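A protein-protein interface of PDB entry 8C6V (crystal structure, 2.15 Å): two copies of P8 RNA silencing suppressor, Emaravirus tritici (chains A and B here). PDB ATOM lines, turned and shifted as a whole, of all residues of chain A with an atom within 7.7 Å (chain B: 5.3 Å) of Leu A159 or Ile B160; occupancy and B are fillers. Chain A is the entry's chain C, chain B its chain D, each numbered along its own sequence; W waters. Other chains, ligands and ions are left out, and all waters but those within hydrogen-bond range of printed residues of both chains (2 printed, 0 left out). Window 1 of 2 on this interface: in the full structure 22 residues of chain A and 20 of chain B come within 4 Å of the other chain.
Leu A159 touches just these residues of chain B: Glu B13, Ile B160 and Leu B163. Of chain A, only Leu A159 comes within 4 Å of Ile B160. Of the printed residues of chain B, Asn A162 touches Val B9 and Glu B13. Of the printed residues of chain B, Asn A158 touches Glu B13. Printed residues of chain B within 4 Å of Glu A13: Asn B162 and Leu B163. Printed residues of chain A within 4 Å of Val B9: Asn A162 and Leu A163. Lys A161 touches none of the printed residues of chain B. The nearest printed residue of chain A that does not touch Leu B163 is Ile A10 (4.3 Å).
Water W1 bridges the side-chain carboxylate (OE1) of Glu B13 and the backbone carbonyl oxygen (O) of Met A155. Water W2 bridges OE1 of Glu B13 (2.9 Å) and OD1 of Asn A162 (3.4 Å).
Among the printed residues, merely in contact across the chains: Met A155 with Val B156 (3.6 Å), Met A155 with Phe B110 (3.6 Å), Val A156 with Val B156 (3.6 Å), Leu A163 with Val B9 (3.7 Å), Leu A159 with Glu B13 (3.8 Å), Leu A163 with Leu B163 (3.9 Å), Asn A158 with Glu B13 (3.9 Å), Glu A13 with Leu B163 (3.9 Å), Leu A159 with Leu B163 (3.9 Å), Leu A159 with Ile B160 (3.9 Å) and Asn A162 with Val B9 (3.98 Å).
O of Asn A158 lies close to OD1 of Asn A162 (3.3 Å). The backbone carbonyl oxygen of Asn B158 lies close to the side-chain amide nitrogen of Asn B162 (3.4 Å).
Of the 16 printed residues of chain A, 7 touch a printed residue of chain B. Printed residues of chain A that touch a printed residue of chain B: Glu A13, Met A155, Val A156, Asn A158, Leu A159, Asn A162 and Leu A163. Among the printed residues, 13 pairs touch across the chains. Among the printed residues, no Asp or Glu carboxylate lies within 4 Å of a Lys or Arg side-chain nitrogen of the other chain.
ND2 of Asn B162 lies within hydrogen-bond range of OE2 of Glu A13, 3.1 Å away. The side-chain carboxylate of Glu B13 lies close to the side-chain amide oxygen of Asn A162 (3.1 Å).
Glu A13 touches Leu B163, but with the chains exchanged Leu A163 does not touch Glu B13 (6.1 Å). Val A156 touches its own counterpart, Val B156. Leu A159 touches Ile B160, but with the chains exchanged Ile A160 does not touch Leu B159 (4.2 Å). Leu A159 touches Leu B163, but with the chains exchanged Leu A163 does not touch Leu B159 (7.0 Å).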
ATOM      1  N   ILE A  10      39.145   4.883   7.209  1.00  0.00           N
ATOM      2  CA  ILE A  10      38.566   3.647   6.691  1.00  0.00           C
ATOM      3  C   ILE A  10      39.633   2.566   6.561  1.00  0.00           C
ATOM      4  O   ILE A  10      39.417   1.410   6.947  1.00  0.00           O
ATOM      5  CB  ILE A  10      37.862   3.913   5.348  1.00  0.00           C
ATOM      6  CG1 ILE A  10      36.627   4.788   5.568  1.00  0.00           C
ATOM      7  CG2 ILE A  10      37.491   2.606   4.663  1.00  0.00           C
ATOM      8  CD1 ILE A  10      35.915   5.162   4.293  1.00  0.00           C
ATOM      9  N   GLU A  13      40.410   1.010   9.747  1.00  0.00           N
ATOM     10  CA  GLU A  13      39.372   0.092  10.202  1.00  0.00           C
ATOM     11  C   GLU A  13      39.379  -1.207   9.405  1.00  0.00           C
ATOM     12  O   GLU A  13      39.164  -2.284   9.971  1.00  0.00           O
ATOM     13  CB  GLU A  13      38.001   0.764  10.118  1.00  0.00           C
ATOM     14  CG  GLU A  13      36.870  -0.083  10.676  1.00  0.00           C
ATOM     15  CD  GLU A  13      37.085  -0.460  12.130  1.00  0.00           C
ATOM     16  OE1 GLU A  13      37.731   0.320  12.864  1.00  0.00           O
ATOM     17  OE2 GLU A  13      36.610  -1.539  12.539  1.00  0.00           O
ATOM     18  N   VAL A  83      37.338  -1.942  -0.305  1.00  0.00           N
ATOM     19  CA  VAL A  83      36.258  -1.138  -0.868  1.00  0.00           C
ATOM     20  C   VAL A  83      36.887  -0.078  -1.761  1.00  0.00           C
ATOM     21  O   VAL A  83      37.778   0.657  -1.322  1.00  0.00           O
ATOM     22  CB  VAL A  83      35.388  -0.474   0.218  1.00  0.00           C
ATOM     23  CG1 VAL A  83      34.339   0.415  -0.423  1.00  0.00           C
ATOM     24  CG2 VAL A  83      34.727  -1.522   1.102  1.00  0.00           C
ATOM     25  N   GLN A 153      26.204  -7.428   4.275  1.00  0.00           N
ATOM     26  CA  GLN A 153      27.497  -7.233   3.631  1.00  0.00           C
ATOM     27  C   GLN A 153      27.413  -6.185   2.528  1.00  0.00           C
ATOM     28  O   GLN A 153      28.381  -5.452   2.294  1.00  0.00           O
ATOM     29  CB  GLN A 153      28.007  -8.566   3.084  1.00  0.00           C
ATOM     30  CG  GLN A 153      28.212  -9.624   4.159  1.00  0.00           C
ATOM     31  CD  GLN A 153      28.422 -11.015   3.591  1.00  0.00           C
ATOM     32  OE1 GLN A 153      27.693 -11.949   3.924  1.00  0.00           O
ATOM     33  NE2 GLN A 153      29.424 -11.162   2.733  1.00  0.00           N
ATOM     34  N   ILE A 154      26.270  -6.103   1.842  1.00  0.00           N
ATOM     35  CA  ILE A 154      26.035  -5.007   0.905  1.00  0.00           C
ATOM     36  C   ILE A 154      25.984  -3.681   1.653  1.00  0.00           C
ATOM     37  O   ILE A 154      26.587  -2.685   1.236  1.00  0.00           O
ATOM     38  CB  ILE A 154      24.734  -5.241   0.114  1.00  0.00           C
ATOM     39  CG1 ILE A 154      24.843  -6.472  -0.782  1.00  0.00           C
ATOM     40  CG2 ILE A 154      24.380  -4.014  -0.714  1.00  0.00           C
ATOM     41  CD1 ILE A 154      23.552  -6.779  -1.520  1.00  0.00           C
ATOM     42  N   MET A 155      25.250  -3.654   2.769  1.00  0.00           N
ATOM     43  CA  MET A 155      25.030  -2.409   3.498  1.00  0.00           C
ATOM     44  C   MET A 155      26.340  -1.811   3.995  1.00  0.00           C
ATOM     45  O   MET A 155      26.543  -0.594   3.916  1.00  0.00           O
ATOM     46  CB  MET A 155      24.073  -2.659   4.662  1.00  0.00           C
ATOM     47  CG  MET A 155      23.853  -1.465   5.572  1.00  0.00           C
ATOM     48  SD  MET A 155      22.799  -1.909   6.964  1.00  0.00           S
ATOM     49  CE  MET A 155      23.694  -3.322   7.598  1.00  0.00           C
ATOM     50  N   VAL A 156      27.241  -2.649   4.509  1.00  0.00           N
ATOM     51  CA  VAL A 156      28.528  -2.155   4.990  1.00  0.00           C
ATOM     52  C   VAL A 156      29.366  -1.636   3.828  1.00  0.00           C
ATOM     53  O   VAL A 156      29.975  -0.563   3.911  1.00  0.00           O
ATOM     54  CB  VAL A 156      29.265  -3.253   5.778  1.00  0.00           C
ATOM     55  CG1 VAL A 156      30.773  -3.069   5.682  1.00  0.00           C
ATOM     56  CG2 VAL A 156      28.825  -3.231   7.228  1.00  0.00           C
ATOM     57  N   SER A 157      29.406  -2.388   2.726  1.00  0.00           N
ATOM     58  CA  SER A 157      30.168  -1.945   1.564  1.00  0.00           C
ATOM     59  C   SER A 157      29.600  -0.650   0.994  1.00  0.00           C
ATOM     60  O   SER A 157      30.355   0.246   0.595  1.00  0.00           O
ATOM     61  CB  SER A 157      30.190  -3.047   0.504  1.00  0.00           C
ATOM     62  OG  SER A 157      30.875  -2.628  -0.662  1.00  0.00           O
ATOM     63  N   ASN A 158      28.271  -0.520   0.965  1.00  0.00           N
ATOM     64  CA  ASN A 158      27.664   0.709   0.461  1.00  0.00           C
ATOM     65  C   ASN A 158      27.964   1.893   1.373  1.00  0.00           C
ATOM     66  O   ASN A 158      28.181   3.012   0.893  1.00  0.00           O
ATOM     67  CB  ASN A 158      26.155   0.532   0.298  1.00  0.00           C
ATOM     68  CG  ASN A 158      25.789  -0.237  -0.956  1.00  0.00           C
ATOM     69  OD1 ASN A 158      26.618  -0.430  -1.844  1.00  0.00           O
ATOM     70  ND2 ASN A 158      24.534  -0.667  -1.041  1.00  0.00           N
ATOM     71  N   LEU A 159      27.979   1.666   2.689  1.00  0.00           N
ATOM     72  CA  LEU A 159      28.265   2.752   3.623  1.00  0.00           C
ATOM     73  C   LEU A 159      29.683   3.276   3.436  1.00  0.00           C
ATOM     74  O   LEU A 159      29.913   4.491   3.460  1.00  0.00           O
ATOM     75  CB  LEU A 159      28.047   2.274   5.060  1.00  0.00           C
ATOM     76  CG  LEU A 159      28.236   3.279   6.201  1.00  0.00           C
ATOM     77  CD1 LEU A 159      27.236   3.006   7.313  1.00  0.00           C
ATOM     78  CD2 LEU A 159      29.656   3.230   6.747  1.00  0.00           C
ATOM     79  N   ILE A 160      30.645   2.373   3.244  1.00  0.00           N
ATOM     80  CA  ILE A 160      32.027   2.791   3.044  1.00  0.00           C
ATOM     81  C   ILE A 160      32.189   3.473   1.691  1.00  0.00           C
ATOM     82  O   ILE A 160      32.952   4.437   1.554  1.00  0.00           O
ATOM     83  CB  ILE A 160      32.969   1.584   3.202  1.00  0.00           C
ATOM     84  CG1 ILE A 160      32.856   1.011   4.616  1.00  0.00           C
ATOM     85  CG2 ILE A 160      34.402   1.977   2.901  1.00  0.00           C
ATOM     86  CD1 ILE A 160      33.615  -0.283   4.820  1.00  0.00           C
ATOM     87  N   LYS A 161      31.468   2.995   0.671  1.00  0.00           N
ATOM     88  CA  LYS A 161      31.520   3.643  -0.635  1.00  0.00           C
ATOM     89  C   LYS A 161      30.997   5.074  -0.564  1.00  0.00           C
ATOM     90  O   LYS A 161      31.563   5.980  -1.186  1.00  0.00           O
ATOM     91  CB  LYS A 161      30.725   2.836  -1.660  1.00  0.00           C
ATOM     92  CG  LYS A 161      31.470   1.646  -2.246  1.00  0.00           C
ATOM     93  CD  LYS A 161      30.665   0.997  -3.363  1.00  0.00           C
ATOM     94  CE  LYS A 161      31.518   0.052  -4.195  1.00  0.00           C
ATOM     95  NZ  LYS A 161      31.193  -1.376  -3.927  1.00  0.00           N
ATOM     96  N   ASN A 162      29.920   5.296   0.195  1.00  0.00           N
ATOM     97  CA  ASN A 162      29.375   6.644   0.322  1.00  0.00           C
ATOM     98  C   ASN A 162      30.320   7.558   1.093  1.00  0.00           C
ATOM     99  O   ASN A 162      30.448   8.743   0.764  1.00  0.00           O
ATOM    100  CB  ASN A 162      28.003   6.594   0.993  1.00  0.00           C
ATOM    101  CG  ASN A 162      26.869   6.509  -0.009  1.00  0.00           C
ATOM    102  OD1 ASN A 162      26.622   5.456  -0.599  1.00  0.00           O
ATOM    103  ND2 ASN A 162      26.167   7.620  -0.202  1.00  0.00           N
ATOM    104  N   LEU A 163      30.985   7.028   2.124  1.00  0.00           N
ATOM    105  CA  LEU A 163      32.000   7.808   2.824  1.00  0.00           C
ATOM    106  C   LEU A 163      33.118   8.228   1.879  1.00  0.00           C
ATOM    107  O   LEU A 163      33.570   9.378   1.910  1.00  0.00           O
ATOM    108  CB  LEU A 163      32.569   7.006   3.997  1.00  0.00           C
ATOM    109  CG  LEU A 163      31.683   6.786   5.224  1.00  0.00           C
ATOM    110  CD1 LEU A 163      32.362   5.832   6.193  1.00  0.00           C
ATOM    111  CD2 LEU A 163      31.365   8.106   5.908  1.00  0.00           C
ATOM    112  N   LEU A 164      33.569   7.309   1.022  1.00  0.00           N
ATOM    113  CA  LEU A 164      34.665   7.593   0.105  1.00  0.00           C
ATOM    114  C   LEU A 164      34.274   8.548  -1.017  1.00  0.00           C
ATOM    115  O   LEU A 164      35.164   9.052  -1.711  1.00  0.00           O
ATOM    116  CB  LEU A 164      35.201   6.286  -0.484  1.00  0.00           C
ATOM    117  CG  LEU A 164      35.968   5.399   0.500  1.00  0.00           C
ATOM    118  CD1 LEU A 164      36.268   4.040  -0.112  1.00  0.00           C
ATOM    119  CD2 LEU A 164      37.255   6.089   0.929  1.00  0.00           C
ATOM    120  N   LYS A 165      32.978   8.808  -1.214  1.00  0.00           N
ATOM    121  CA  LYS A 165      32.570   9.810  -2.195  1.00  0.00           C
ATOM    122  C   LYS A 165      33.074  11.196  -1.816  1.00  0.00           C
ATOM    123  O   LYS A 165      33.278  12.043  -2.694  1.00  0.00           O
ATOM    124  CB  LYS A 165      31.048   9.829  -2.342  1.00  0.00           C
ATOM    125  CG  LYS A 165      30.482   8.707  -3.194  1.00  0.00           C
ATOM    126  CD  LYS A 165      28.964   8.761  -3.228  1.00  0.00           C
ATOM    127  CE  LYS A 165      28.396   7.729  -4.187  1.00  0.00           C
ATOM    128  NZ  LYS A 165      26.909   7.660  -4.114  1.00  0.00           N
ATOM    129  N   VAL B   9      27.175  11.352   6.954  1.00  0.00           N
ATOM    130  CA  VAL B   9      26.992  10.336   5.920  1.00  0.00           C
ATOM    131  C   VAL B   9      26.464   9.040   6.526  1.00  0.00           C
ATOM    132  O   VAL B   9      25.612   8.366   5.934  1.00  0.00           O
ATOM    133  CB  VAL B   9      28.310  10.111   5.155  1.00  0.00           C
ATOM    134  CG1 VAL B   9      28.199   8.903   4.229  1.00  0.00           C
ATOM    135  CG2 VAL B   9      28.680  11.356   4.365  1.00  0.00           C
ATOM    136  N   ILE B  10      26.955   8.672   7.711  1.00  0.00           N
ATOM    137  CA  ILE B  10      26.499   7.440   8.348  1.00  0.00           C
ATOM    138  C   ILE B  10      25.024   7.541   8.716  1.00  0.00           C
ATOM    139  O   ILE B  10      24.255   6.592   8.520  1.00  0.00           O
ATOM    140  CB  ILE B  10      27.373   7.115   9.573  1.00  0.00           C
ATOM    141  CG1 ILE B  10      28.749   6.614   9.124  1.00  0.00           C
ATOM    142  CG2 ILE B  10      26.690   6.088  10.466  1.00  0.00           C
ATOM    143  CD1 ILE B  10      29.687   6.287  10.267  1.00  0.00           C
ATOM    144  N   GLU B  13      23.174   7.030   5.569  1.00  0.00           N
ATOM    145  CA  GLU B  13      23.184   5.640   5.121  1.00  0.00           C
ATOM    146  C   GLU B  13      22.249   4.777   5.960  1.00  0.00           C
ATOM    147  O   GLU B  13      21.535   3.924   5.421  1.00  0.00           O
ATOM    148  CB  GLU B  13      24.608   5.085   5.159  1.00  0.00           C
ATOM    149  CG  GLU B  13      25.433   5.449   3.940  1.00  0.00           C
ATOM    150  CD  GLU B  13      24.866   4.857   2.665  1.00  0.00           C
ATOM    151  OE1 GLU B  13      24.686   3.623   2.611  1.00  0.00           O
ATOM    152  OE2 GLU B  13      24.586   5.627   1.722  1.00  0.00           O
ATOM    153  N   LEU B  14      22.244   4.975   7.280  1.00  0.00           N
ATOM    154  CA  LEU B  14      21.313   4.233   8.123  1.00  0.00           C
ATOM    155  C   LEU B  14      19.871   4.552   7.757  1.00  0.00           C
ATOM    156  O   LEU B  14      19.007   3.666   7.772  1.00  0.00           O
ATOM    157  CB  LEU B  14      21.578   4.540   9.596  1.00  0.00           C
ATOM    158  CG  LEU B  14      22.956   4.128  10.117  1.00  0.00           C
ATOM    159  CD1 LEU B  14      23.094   4.495  11.584  1.00  0.00           C
ATOM    160  CD2 LEU B  14      23.200   2.639   9.901  1.00  0.00           C
ATOM    161  N   VAL B  83      23.127   3.143  15.620  1.00  0.00           N
ATOM    162  CA  VAL B  83      24.471   2.906  16.140  1.00  0.00           C
ATOM    163  C   VAL B  83      24.863   4.107  16.989  1.00  0.00           C
ATOM    164  O   VAL B  83      24.789   5.249  16.525  1.00  0.00           O
ATOM    165  CB  VAL B  83      25.506   2.685  15.017  1.00  0.00           C
ATOM    166  CG1 VAL B  83      26.888   2.468  15.610  1.00  0.00           C
ATOM    167  CG2 VAL B  83      25.109   1.507  14.133  1.00  0.00           C
ATOM    168  N   PHE B 110      20.147  -4.845  13.111  1.00  0.00           N
ATOM    169  CA  PHE B 110      20.316  -5.140  11.687  1.00  0.00           C
ATOM    170  C   PHE B 110      19.750  -6.512  11.329  1.00  0.00           C
ATOM    171  O   PHE B 110      20.352  -7.276  10.572  1.00  0.00           O
ATOM    172  CB  PHE B 110      21.785  -5.025  11.270  1.00  0.00           C
ATOM    173  CG  PHE B 110      22.395  -3.689  11.582  1.00  0.00           C
ATOM    174  CD1 PHE B 110      22.159  -2.600  10.762  1.00  0.00           C
ATOM    175  CD2 PHE B 110      23.196  -3.521  12.699  1.00  0.00           C
ATOM    176  CE1 PHE B 110      22.714  -1.367  11.049  1.00  0.00           C
ATOM    177  CE2 PHE B 110      23.755  -2.289  12.989  1.00  0.00           C
ATOM    178  CZ  PHE B 110      23.511  -1.212  12.163  1.00  0.00           C
ATOM    179  N   MET B 155      29.164  -7.774  13.644  1.00  0.00           N
ATOM    180  CA  MET B 155      30.269  -7.270  12.834  1.00  0.00           C
ATOM    181  C   MET B 155      29.908  -5.933  12.199  1.00  0.00           C
ATOM    182  O   MET B 155      30.726  -5.006  12.175  1.00  0.00           O
ATOM    183  CB  MET B 155      30.642  -8.298  11.763  1.00  0.00           C
ATOM    184  CG  MET B 155      31.852  -7.932  10.904  1.00  0.00           C
ATOM    185  SD  MET B 155      31.479  -6.817   9.530  1.00  0.00           S
ATOM    186  CE  MET B 155      30.119  -7.683   8.753  1.00  0.00           C
ATOM    187  N   VAL B 156      28.685  -5.819  11.681  1.00  0.00           N
ATOM    188  CA  VAL B 156      28.236  -4.567  11.075  1.00  0.00           C
ATOM    189  C   VAL B 156      28.190  -3.459  12.118  1.00  0.00           C
ATOM    190  O   VAL B 156      28.671  -2.342  11.889  1.00  0.00           O
ATOM    191  CB  VAL B 156      26.862  -4.760  10.408  1.00  0.00           C
ATOM    192  CG1 VAL B 156      26.251  -3.412  10.061  1.00  0.00           C
ATOM    193  CG2 VAL B 156      26.990  -5.637   9.172  1.00  0.00           C
ATOM    194  N   SER B 157      27.606  -3.754  13.281  1.00  0.00           N
ATOM    195  CA  SER B 157      27.463  -2.741  14.320  1.00  0.00           C
ATOM    196  C   SER B 157      28.819  -2.281  14.842  1.00  0.00           C
ATOM    197  O   SER B 157      29.013  -1.091  15.114  1.00  0.00           O
ATOM    198  CB  SER B 157      26.602  -3.284  15.459  1.00  0.00           C
ATOM    199  OG  SER B 157      26.402  -2.297  16.455  1.00  0.00           O
ATOM    200  N   ASN B 158      29.772  -3.206  14.985  1.00  0.00           N
ATOM    201  CA  ASN B 158      31.083  -2.827  15.509  1.00  0.00           C
ATOM    202  C   ASN B 158      31.852  -1.968  14.516  1.00  0.00           C
ATOM    203  O   ASN B 158      32.555  -1.033  14.915  1.00  0.00           O
ATOM    204  CB  ASN B 158      31.895  -4.068  15.876  1.00  0.00           C
ATOM    205  CG  ASN B 158      31.434  -4.705  17.167  1.00  0.00           C
ATOM    206  OD1 ASN B 158      30.693  -4.102  17.942  1.00  0.00           O
ATOM    207  ND2 ASN B 158      31.877  -5.932  17.410  1.00  0.00           N
ATOM    208  N   LEU B 159      31.734  -2.268  13.220  1.00  0.00           N
ATOM    209  CA  LEU B 159      32.472  -1.510  12.215  1.00  0.00           C
ATOM    210  C   LEU B 159      31.987  -0.066  12.156  1.00  0.00           C
ATOM    211  O   LEU B 159      32.794   0.871  12.117  1.00  0.00           O
ATOM    212  CB  LEU B 159      32.346  -2.187  10.848  1.00  0.00           C
ATOM    213  CG  LEU B 159      33.176  -1.604   9.700  1.00  0.00           C
ATOM    214  CD1 LEU B 159      33.754  -2.716   8.839  1.00  0.00           C
ATOM    215  CD2 LEU B 159      32.345  -0.657   8.846  1.00  0.00           C
ATOM    216  N   ILE B 160      30.667   0.134  12.148  1.00  0.00           N
ATOM    217  CA  ILE B 160      30.118   1.486  12.112  1.00  0.00           C
ATOM    218  C   ILE B 160      30.442   2.228  13.402  1.00  0.00           C
ATOM    219  O   ILE B 160      30.714   3.435  13.391  1.00  0.00           O
ATOM    220  CB  ILE B 160      28.603   1.439  11.849  1.00  0.00           C
ATOM    221  CG1 ILE B 160      28.311   0.653  10.570  1.00  0.00           C
ATOM    222  CG2 ILE B 160      28.037   2.845  11.757  1.00  0.00           C
ATOM    223  CD1 ILE B 160      26.838   0.455  10.302  1.00  0.00           C
ATOM    224  N   LYS B 161      30.433   1.515  14.531  1.00  0.00           N
ATOM    225  CA  LYS B 161      30.766   2.138  15.807  1.00  0.00           C
ATOM    226  C   LYS B 161      32.217   2.597  15.833  1.00  0.00           C
ATOM    227  O   LYS B 161      32.530   3.665  16.374  1.00  0.00           O
ATOM    228  CB  LYS B 161      30.488   1.161  16.949  1.00  0.00           C
ATOM    229  CG  LYS B 161      30.453   1.801  18.323  1.00  0.00           C
ATOM    230  CD  LYS B 161      29.960   0.810  19.365  1.00  0.00           C
ATOM    231  CE  LYS B 161      28.601   0.235  18.976  1.00  0.00           C
ATOM    232  NZ  LYS B 161      28.018  -0.652  20.027  1.00  0.00           N
ATOM    233  N   ASN B 162      33.118   1.808  15.241  1.00  0.00           N
ATOM    234  CA  ASN B 162      34.527   2.187  15.214  1.00  0.00           C
ATOM    235  C   ASN B 162      34.779   3.349  14.265  1.00  0.00           C
ATOM    236  O   ASN B 162      35.660   4.177  14.525  1.00  0.00           O
ATOM    237  CB  ASN B 162      35.390   0.989  14.826  1.00  0.00           C
ATOM    238  CG  ASN B 162      35.424  -0.076  15.899  1.00  0.00           C
ATOM    239  OD1 ASN B 162      35.079   0.175  17.055  1.00  0.00           O
ATOM    240  ND2 ASN B 162      35.848  -1.276  15.524  1.00  0.00           N
ATOM    241  N   LEU B 163      34.021   3.435  13.169  1.00  0.00           N
ATOM    242  CA  LEU B 163      34.166   4.569  12.263  1.00  0.00           C
ATOM    243  C   LEU B 163      33.701   5.865  12.912  1.00  0.00           C
ATOM    244  O   LEU B 163      34.172   6.947  12.543  1.00  0.00           O
ATOM    245  CB  LEU B 163      33.388   4.319  10.971  1.00  0.00           C
ATOM    246  CG  LEU B 163      33.912   3.236  10.026  1.00  0.00           C
ATOM    247  CD1 LEU B 163      32.979   3.077   8.836  1.00  0.00           C
ATOM    248  CD2 LEU B 163      35.327   3.561   9.562  1.00  0.00           C
ATOM    249  N   LEU B 164      32.789   5.777  13.880  1.00  0.00           N
ATOM    250  CA  LEU B 164      32.237   6.948  14.547  1.00  0.00           C
ATOM    251  C   LEU B 164      33.058   7.410  15.744  1.00  0.00           C
ATOM    252  O   LEU B 164      32.757   8.471  16.301  1.00  0.00           O
ATOM    253  CB  LEU B 164      30.803   6.667  15.007  1.00  0.00           C
ATOM    254  CG  LEU B 164      29.698   6.692  13.948  1.00  0.00           C
ATOM    255  CD1 LEU B 164      28.440   6.017  14.476  1.00  0.00           C
ATOM    256  CD2 LEU B 164      29.404   8.124  13.536  1.00  0.00           C
HETATM  257  O   HOH W   1      24.249   1.179   3.191  1.00  0.00           O
HETATM  258  O   HOH W   2      23.997   3.399  -0.179  1.00  0.00           O
